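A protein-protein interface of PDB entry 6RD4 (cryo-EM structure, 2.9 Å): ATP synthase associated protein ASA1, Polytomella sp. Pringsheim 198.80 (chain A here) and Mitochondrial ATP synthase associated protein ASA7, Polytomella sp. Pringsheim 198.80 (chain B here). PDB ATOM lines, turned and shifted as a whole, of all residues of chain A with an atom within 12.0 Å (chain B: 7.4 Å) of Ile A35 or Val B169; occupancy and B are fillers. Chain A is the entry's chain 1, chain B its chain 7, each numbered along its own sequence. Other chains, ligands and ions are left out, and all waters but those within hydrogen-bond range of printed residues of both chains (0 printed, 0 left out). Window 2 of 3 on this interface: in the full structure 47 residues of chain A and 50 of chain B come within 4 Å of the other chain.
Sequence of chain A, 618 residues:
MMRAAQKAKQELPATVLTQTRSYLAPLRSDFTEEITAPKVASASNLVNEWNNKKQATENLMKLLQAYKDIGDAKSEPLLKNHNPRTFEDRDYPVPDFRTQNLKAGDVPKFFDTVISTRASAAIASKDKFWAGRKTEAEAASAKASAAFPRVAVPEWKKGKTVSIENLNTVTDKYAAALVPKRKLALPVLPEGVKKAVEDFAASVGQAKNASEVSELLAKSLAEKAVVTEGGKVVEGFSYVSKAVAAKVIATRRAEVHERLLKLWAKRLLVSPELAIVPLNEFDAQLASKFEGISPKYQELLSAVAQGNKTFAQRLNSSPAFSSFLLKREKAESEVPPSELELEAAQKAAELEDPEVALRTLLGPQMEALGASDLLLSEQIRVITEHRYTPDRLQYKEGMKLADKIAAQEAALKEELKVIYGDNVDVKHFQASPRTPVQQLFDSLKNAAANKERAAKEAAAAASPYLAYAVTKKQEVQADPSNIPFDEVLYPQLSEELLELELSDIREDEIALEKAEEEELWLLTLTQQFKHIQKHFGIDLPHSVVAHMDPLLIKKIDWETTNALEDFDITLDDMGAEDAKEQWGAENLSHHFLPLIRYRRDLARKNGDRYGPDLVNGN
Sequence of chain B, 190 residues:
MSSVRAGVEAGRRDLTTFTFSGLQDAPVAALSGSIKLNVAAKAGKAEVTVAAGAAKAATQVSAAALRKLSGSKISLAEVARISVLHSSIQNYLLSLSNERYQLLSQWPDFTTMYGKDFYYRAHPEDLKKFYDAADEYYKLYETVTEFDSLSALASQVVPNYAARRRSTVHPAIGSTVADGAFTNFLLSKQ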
ATOM      1  N   ASP A  30       2.955  -9.123 -18.002  1.00  0.00           N
ATOM      2  CA  ASP A  30       2.460 -10.325 -17.363  1.00  0.00           C
ATOM      3  C   ASP A  30       2.457 -11.437 -18.389  1.00  0.00           C
ATOM      4  O   ASP A  30       2.420 -11.191 -19.594  1.00  0.00           O
ATOM      5  CB  ASP A  30       1.061 -10.146 -16.785  1.00  0.00           C
ATOM      6  CG  ASP A  30       0.018  -9.936 -17.846  1.00  0.00           C
ATOM      7  OD1 ASP A  30       0.120  -8.938 -18.571  1.00  0.00           O
ATOM      8  OD2 ASP A  30      -0.894 -10.774 -17.975  1.00  0.00           O
ATOM      9  N   PHE A  31       2.482 -12.663 -17.898  1.00  0.00           N
ATOM     10  CA  PHE A  31       2.701 -13.827 -18.727  1.00  0.00           C
ATOM     11  C   PHE A  31       1.433 -14.659 -18.805  1.00  0.00           C
ATOM     12  O   PHE A  31       0.536 -14.547 -17.971  1.00  0.00           O
ATOM     13  CB  PHE A  31       3.855 -14.655 -18.172  1.00  0.00           C
ATOM     14  CG  PHE A  31       5.193 -14.006 -18.318  1.00  0.00           C
ATOM     15  CD1 PHE A  31       6.030 -14.361 -19.346  1.00  0.00           C
ATOM     16  CD2 PHE A  31       5.620 -13.045 -17.427  1.00  0.00           C
ATOM     17  CE1 PHE A  31       7.251 -13.773 -19.481  1.00  0.00           C
ATOM     18  CE2 PHE A  31       6.840 -12.452 -17.570  1.00  0.00           C
ATOM     19  CZ  PHE A  31       7.652 -12.816 -18.592  1.00  0.00           C
ATOM     20  N   THR A  32       1.355 -15.484 -19.831  1.00  0.00           N
ATOM     21  CA  THR A  32       0.238 -16.396 -20.016  1.00  0.00           C
ATOM     22  C   THR A  32       0.701 -17.783 -19.609  1.00  0.00           C
ATOM     23  O   THR A  32       1.503 -18.404 -20.304  1.00  0.00           O
ATOM     24  CB  THR A  32      -0.249 -16.377 -21.459  1.00  0.00           C
ATOM     25  OG1 THR A  32      -0.729 -15.069 -21.768  1.00  0.00           O
ATOM     26  CG2 THR A  32      -1.370 -17.344 -21.652  1.00  0.00           C
ATOM     27  N   GLU A  33       0.208 -18.266 -18.477  1.00  0.00           N
ATOM     28  CA  GLU A  33       0.607 -19.581 -18.009  1.00  0.00           C
ATOM     29  C   GLU A  33      -0.238 -20.699 -18.581  1.00  0.00           C
ATOM     30  O   GLU A  33       0.254 -21.814 -18.731  1.00  0.00           O
ATOM     31  CB  GLU A  33       0.573 -19.622 -16.489  1.00  0.00           C
ATOM     32  CG  GLU A  33       1.812 -19.034 -15.864  1.00  0.00           C
ATOM     33  CD  GLU A  33       1.704 -17.551 -15.649  1.00  0.00           C
ATOM     34  OE1 GLU A  33       0.631 -16.988 -15.945  1.00  0.00           O
ATOM     35  OE2 GLU A  33       2.691 -16.943 -15.185  1.00  0.00           O
ATOM     36  N   GLU A  34      -1.484 -20.435 -18.922  1.00  0.00           N
ATOM     37  CA  GLU A  34      -2.313 -21.447 -19.539  1.00  0.00           C
ATOM     38  C   GLU A  34      -1.963 -21.598 -21.012  1.00  0.00           C
ATOM     39  O   GLU A  34      -1.183 -20.837 -21.573  1.00  0.00           O
ATOM     40  CB  GLU A  34      -3.787 -21.090 -19.382  1.00  0.00           C
ATOM     41  CG  GLU A  34      -4.187 -19.784 -20.060  1.00  0.00           C
ATOM     42  CD  GLU A  34      -4.025 -18.562 -19.176  1.00  0.00           C
ATOM     43  OE1 GLU A  34      -3.446 -18.684 -18.074  1.00  0.00           O
ATOM     44  OE2 GLU A  34      -4.473 -17.474 -19.589  1.00  0.00           O
ATOM     45  N   ILE A  35      -2.514 -22.628 -21.630  1.00  0.00           N
ATOM     46  CA  ILE A  35      -2.514 -22.778 -23.073  1.00  0.00           C
ATOM     47  C   ILE A  35      -3.961 -23.070 -23.422  1.00  0.00           C
ATOM     48  O   ILE A  35      -4.414 -24.213 -23.323  1.00  0.00           O
ATOM     49  CB  ILE A  35      -1.584 -23.885 -23.566  1.00  0.00           C
ATOM     50  CG1 ILE A  35      -0.147 -23.579 -23.200  1.00  0.00           C
ATOM     51  CG2 ILE A  35      -1.662 -24.023 -25.056  1.00  0.00           C
ATOM     52  CD1 ILE A  35       0.791 -24.643 -23.604  1.00  0.00           C
ATOM     53  N   THR A  36      -4.701 -22.038 -23.793  1.00  0.00           N
ATOM     54  CA  THR A  36      -6.127 -22.139 -24.029  1.00  0.00           C
ATOM     55  C   THR A  36      -6.454 -21.795 -25.469  1.00  0.00           C
ATOM     56  O   THR A  36      -5.594 -21.411 -26.257  1.00  0.00           O
ATOM     57  CB  THR A  36      -6.903 -21.220 -23.088  1.00  0.00           C
ATOM     58  OG1 THR A  36      -6.335 -19.909 -23.138  1.00  0.00           O
ATOM     59  CG2 THR A  36      -6.880 -21.739 -21.678  1.00  0.00           C
ATOM     60  N   ALA A  37      -7.718 -21.988 -25.804  1.00  0.00           N
ATOM     61  CA  ALA A  37      -8.247 -21.514 -27.061  1.00  0.00           C
ATOM     62  C   ALA A  37      -8.472 -20.007 -26.966  1.00  0.00           C
ATOM     63  O   ALA A  37      -8.726 -19.484 -25.880  1.00  0.00           O
ATOM     64  CB  ALA A  37      -9.548 -22.240 -27.383  1.00  0.00           C
ATOM     65  N   PRO A  38      -8.373 -19.282 -28.077  1.00  0.00           N
ATOM     66  CA  PRO A  38      -8.285 -17.824 -27.978  1.00  0.00           C
ATOM     67  C   PRO A  38      -9.583 -17.034 -27.859  1.00  0.00           C
ATOM     68  O   PRO A  38      -9.524 -15.822 -28.077  1.00  0.00           O
ATOM     69  CB  PRO A  38      -7.559 -17.447 -29.270  1.00  0.00           C
ATOM     70  CG  PRO A  38      -7.039 -18.681 -29.817  1.00  0.00           C
ATOM     71  CD  PRO A  38      -7.959 -19.731 -29.411  1.00  0.00           C
ATOM     72  N   LYS A  39     -10.720 -17.661 -27.531  1.00  0.00           N
ATOM     73  CA  LYS A  39     -11.988 -16.988 -27.187  1.00  0.00           C
ATOM     74  C   LYS A  39     -12.538 -16.133 -28.337  1.00  0.00           C
ATOM     75  O   LYS A  39     -12.530 -14.906 -28.288  1.00  0.00           O
ATOM     76  CB  LYS A  39     -11.845 -16.127 -25.929  1.00  0.00           C
ATOM     77  CG  LYS A  39     -11.831 -16.893 -24.641  1.00  0.00           C
ATOM     78  CD  LYS A  39     -13.180 -17.498 -24.338  1.00  0.00           C
ATOM     79  CE  LYS A  39     -13.108 -18.394 -23.121  1.00  0.00           C
ATOM     80  NZ  LYS A  39     -12.210 -19.560 -23.342  1.00  0.00           N
ATOM     81  N   ARG B 164      -0.912 -12.784 -24.730  1.00  0.00           N
ATOM     82  CA  ARG B 164      -1.006 -14.193 -25.069  1.00  0.00           C
ATOM     83  C   ARG B 164       0.249 -14.678 -25.752  1.00  0.00           C
ATOM     84  O   ARG B 164       0.521 -15.879 -25.768  1.00  0.00           O
ATOM     85  CB  ARG B 164      -2.200 -14.442 -25.965  1.00  0.00           C
ATOM     86  CG  ARG B 164      -3.498 -14.306 -25.263  1.00  0.00           C
ATOM     87  CD  ARG B 164      -4.618 -14.577 -26.208  1.00  0.00           C
ATOM     88  NE  ARG B 164      -4.337 -15.728 -27.040  1.00  0.00           N
ATOM     89  CZ  ARG B 164      -4.637 -16.970 -26.700  1.00  0.00           C
ATOM     90  NH1 ARG B 164      -4.348 -17.964 -27.516  1.00  0.00           N
ATOM     91  NH2 ARG B 164      -5.223 -17.214 -25.544  1.00  0.00           N
ATOM     92  N   ARG B 166       3.216 -13.569 -24.784  1.00  0.00           N
ATOM     93  CA  ARG B 166       4.179 -13.690 -23.697  1.00  0.00           C
ATOM     94  C   ARG B 166       3.904 -14.930 -22.878  1.00  0.00           C
ATOM     95  O   ARG B 166       3.771 -14.887 -21.669  1.00  0.00           O
ATOM     96  CB  ARG B 166       4.147 -12.452 -22.823  1.00  0.00           C
ATOM     97  CG  ARG B 166       5.017 -11.353 -23.321  1.00  0.00           C
ATOM     98  CD  ARG B 166       5.195 -10.321 -22.255  1.00  0.00           C
ATOM     99  NE  ARG B 166       3.931  -9.948 -21.645  1.00  0.00           N
ATOM    100  CZ  ARG B 166       3.124  -9.012 -22.118  1.00  0.00           C
ATOM    101  NH1 ARG B 166       1.996  -8.735 -21.497  1.00  0.00           N
ATOM    102  NH2 ARG B 166       3.440  -8.354 -23.209  1.00  0.00           N
ATOM    103  N   SER B 167       3.816 -16.059 -23.557  1.00  0.00           N
ATOM    104  CA  SER B 167       3.537 -17.312 -22.905  1.00  0.00           C
ATOM    105  C   SER B 167       4.813 -17.826 -22.279  1.00  0.00           C
ATOM    106  O   SER B 167       5.909 -17.561 -22.763  1.00  0.00           O
ATOM    107  CB  SER B 167       2.987 -18.310 -23.911  1.00  0.00           C
ATOM    108  OG  SER B 167       2.612 -19.517 -23.295  1.00  0.00           O
ATOM    109  N   THR B 168       4.669 -18.541 -21.179  1.00  0.00           N
ATOM    110  CA  THR B 168       5.814 -19.133 -20.517  1.00  0.00           C
ATOM    111  C   THR B 168       6.275 -20.413 -21.187  1.00  0.00           C
ATOM    112  O   THR B 168       7.282 -20.984 -20.767  1.00  0.00           O
ATOM    113  CB  THR B 168       5.476 -19.423 -19.067  1.00  0.00           C
ATOM    114  OG1 THR B 168       4.393 -20.354 -19.019  1.00  0.00           O
ATOM    115  CG2 THR B 168       5.063 -18.163 -18.379  1.00  0.00           C
ATOM    116  N   VAL B 169       5.569 -20.873 -22.211  1.00  0.00           N
ATOM    117  CA  VAL B 169       5.935 -22.081 -22.927  1.00  0.00           C
ATOM    118  C   VAL B 169       6.636 -21.706 -24.221  1.00  0.00           C
ATOM    119  O   VAL B 169       7.800 -22.050 -24.422  1.00  0.00           O
ATOM    120  CB  VAL B 169       4.701 -22.945 -23.192  1.00  0.00           C
ATOM    121  CG1 VAL B 169       5.074 -24.143 -23.968  1.00  0.00           C
ATOM    122  CG2 VAL B 169       4.096 -23.355 -21.905  1.00  0.00           C
ATOM    123  N   HIS B 170       5.944 -20.986 -25.096  1.00  0.00           N
ATOM    124  CA  HIS B 170       6.469 -20.574 -26.389  1.00  0.00           C
ATOM    125  C   HIS B 170       5.563 -19.487 -26.933  1.00  0.00           C
ATOM    126  O   HIS B 170       4.374 -19.476 -26.612  1.00  0.00           O
ATOM    127  CB  HIS B 170       6.528 -21.751 -27.368  1.00  0.00           C
ATOM    128  CG  HIS B 170       7.407 -21.515 -28.552  1.00  0.00           C
ATOM    129  ND1 HIS B 170       8.723 -21.893 -28.589  1.00  0.00           N
ATOM    130  CD2 HIS B 170       7.150 -20.950 -29.749  1.00  0.00           C
ATOM    131  CE1 HIS B 170       9.241 -21.558 -29.754  1.00  0.00           C
ATOM    132  NE2 HIS B 170       8.307 -20.981 -30.475  1.00  0.00           N
ATOM    133  N   PRO B 171       6.087 -18.552 -27.729  1.00  0.00           N
ATOM    134  CA  PRO B 171       5.207 -17.585 -28.399  1.00  0.00           C
ATOM    135  C   PRO B 171       4.216 -18.197 -29.363  1.00  0.00           C
ATOM    136  O   PRO B 171       3.108 -17.683 -29.499  1.00  0.00           O
ATOM    137  CB  PRO B 171       6.198 -16.693 -29.139  1.00  0.00           C
ATOM    138  CG  PRO B 171       7.403 -16.787 -28.377  1.00  0.00           C
ATOM    139  CD  PRO B 171       7.485 -18.115 -27.769  1.00  0.00           C
ATOM    140  N   ALA B 172       4.580 -19.287 -30.030  1.00  0.00           N
ATOM    141  CA  ALA B 172       3.784 -19.911 -31.069  1.00  0.00           C
ATOM    142  C   ALA B 172       3.041 -21.137 -30.591  1.00  0.00           C
ATOM    143  O   ALA B 172       2.604 -21.939 -31.416  1.00  0.00           O
ATOM    144  CB  ALA B 172       4.670 -20.293 -32.245  1.00  0.00           C
ATOM    145  N   ILE B 173       2.893 -21.313 -29.307  1.00  0.00           N
ATOM    146  CA  ILE B 173       2.233 -22.506 -28.800  1.00  0.00           C
ATOM    147  C   ILE B 173       0.731 -22.361 -28.982  1.00  0.00           C
ATOM    148  O   ILE B 173       0.190 -21.254 -29.044  1.00  0.00           O
ATOM    149  CB  ILE B 173       2.633 -22.754 -27.331  1.00  0.00           C
ATOM    150  CG1 ILE B 173       2.436 -24.214 -26.938  1.00  0.00           C
ATOM    151  CG2 ILE B 173       1.907 -21.831 -26.387  1.00  0.00           C
ATOM    152  CD1 ILE B 173       3.127 -25.180 -27.808  1.00  0.00           C
ATOM    153  N   GLY B 174       0.052 -23.490 -29.147  1.00  0.00           N
ATOM    154  CA  GLY B 174      -1.390 -23.508 -29.216  1.00  0.00           C
ATOM    155  C   GLY B 174      -1.914 -24.810 -28.662  1.00  0.00           C
ATOM    156  O   GLY B 174      -1.153 -25.629 -28.166  1.00  0.00           O
ATOM    157  N   SER B 175      -3.225 -24.995 -28.765  1.00  0.00           N
ATOM    158  CA  SER B 175      -3.816 -26.185 -28.170  1.00  0.00           C
ATOM    159  C   SER B 175      -3.550 -27.430 -28.991  1.00  0.00           C
ATOM    160  O   SER B 175      -3.314 -28.490 -28.416  1.00  0.00           O
ATOM    161  CB  SER B 175      -5.312 -26.008 -27.979  1.00  0.00           C
ATOM    162  OG  SER B 175      -5.574 -25.082 -26.949  1.00  0.00           O
ATOM    163  N   THR B 176      -3.580 -27.333 -30.319  1.00  0.00           N
ATOM    164  CA  THR B 176      -3.431 -28.523 -31.147  1.00  0.00           C
ATOM    165  C   THR B 176      -2.035 -29.108 -31.039  1.00  0.00           C
ATOM    166  O   THR B 176      -1.866 -30.328 -31.060  1.00  0.00           O
ATOM    167  CB  THR B 176      -3.751 -28.192 -32.596  1.00  0.00           C
ATOM    168  OG1 THR B 176      -4.960 -27.436 -32.644  1.00  0.00           O
ATOM    169  CG2 THR B 176      -3.924 -29.448 -33.414  1.00  0.00           C
ATOM    170  N   VAL B 177      -1.022 -28.262 -30.902  1.00  0.00           N
ATOM    171  CA  VAL B 177       0.329 -28.769 -30.707  1.00  0.00           C
ATOM    172  C   VAL B 177       0.491 -29.302 -29.296  1.00  0.00           C
ATOM    173  O   VAL B 177       1.025 -30.392 -29.093  1.00  0.00           O
ATOM    174  CB  VAL B 177       1.355 -27.675 -31.032  1.00  0.00           C
ATOM    175  CG1 VAL B 177       2.721 -28.065 -30.587  1.00  0.00           C
ATOM    176  CG2 VAL B 177       1.370 -27.431 -32.497  1.00  0.00           C
ATOM    177  N   ALA B 178      -0.008 -28.578 -28.304  1.00  0.00           N
ATOM    178  CA  ALA B 178       0.159 -29.005 -26.925  1.00  0.00           C
ATOM    179  C   ALA B 178      -0.724 -30.184 -26.555  1.00  0.00           C
ATOM    180  O   ALA B 178      -0.481 -30.813 -25.527  1.00  0.00           O
ATOM    181  CB  ALA B 178      -0.118 -27.850 -25.977  1.00  0.00           C
ATOM    182  N   ASP B 179      -1.747 -30.487 -27.349  1.00  0.00           N
ATOM    183  CA  ASP B 179      -2.465 -31.741 -27.174  1.00  0.00           C
ATOM    184  C   ASP B 179      -1.747 -32.869 -27.877  1.00  0.00           C
ATOM    185  O   ASP B 179      -1.734 -33.999 -27.389  1.00  0.00           O
ATOM    186  CB  ASP B 179      -3.883 -31.628 -27.712  1.00  0.00           C
ATOM    187  CG  ASP B 179      -4.748 -30.738 -26.868  1.00  0.00           C
ATOM    188  OD1 ASP B 179      -4.266 -30.254 -25.827  1.00  0.00           O
ATOM    189  OD2 ASP B 179      -5.910 -30.504 -27.253  1.00  0.00           O
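Of chain B, only Val B169 (3.9 Å), Ile B173 (3.7 Å), Gly B174 (3.5 Å) and Ser B175 (3.9 Å) come within 4 Å of Ile A35. Val B169 touches just one residue of chain A: Ile A35. Of chain A, only Ile A35 (3.7 Å) comes within 4 Å of Ile B173. Gly B174 touches just one residue of chain A: Ile A35. Of chain A, only Ile A35 (3.9 Å), Thr A36 (3.7 Å) and Ala A37 (3.9 Å) come within 4 Å of Ser B175. No residue of chain A comes within 4 Å of Ala B178. Of the printed residues of chain B, Phe A31 touches Arg B166 and Thr B168. Of the printed residues of chain B, Asp A30 touches Arg B166 (2.8 Å). Of the printed residues of chain B, Thr A36 touches Arg B164 and Ser B175. The nearest residue of chain B that does not touch Ile A35 is Ala B178 (4.1 Å). The nearest residue of chain A that does not touch Val B169 is Thr A32 (5.1 Å).
The side-chain carboxylate (OD1) of Asp A30 is in salt-bridge range of the guanidinium group (NH1) of Arg B166, at 3.5 Å. N of Thr A32 sits at hydrogen-bond distance from O of Arg B166 (3.1 Å). The backbone NH of Thr B168 sits at hydrogen-bond distance from the backbone carbonyl oxygen of Thr A32 (3.3 Å). The side-chain hydroxyl (OG) of Ser B167 sits at hydrogen-bond distance from the backbone carbonyl oxygen (O) of Thr A32, at 3.4 Å.
Hydrophobic or aromatic side chains of chain A that line the printed part of chain B: Phe A31, Ile A35 and Pro A38. Among the printed residues, 16 pairs touch across the chains.
Phe A31 touches Arg B166 (CD1 to O, 3.3 Å). Phe A31 touches Thr B168. Arg B164 touches Thr A32. Glu A33 touches Thr B168 (CA to OG1, 3.99 Å). CG2 of Val B169 touches CD1 of Ile A35, at 3.9 Å. CD1 of Ile A35 touches CG1 of Ile B173 (3.7 Å). O of Gly B174 touches CG2 of Ile A35, at 3.5 Å. O of Ile A35 touches OG of Ser B175, 3.9 Å away. Thr A36 touches Ser B175. Arg B164 touches Pro A38 (NH1 to CG, 3.6 Å).
OG of Ser B167 sits close to N of Val B169.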
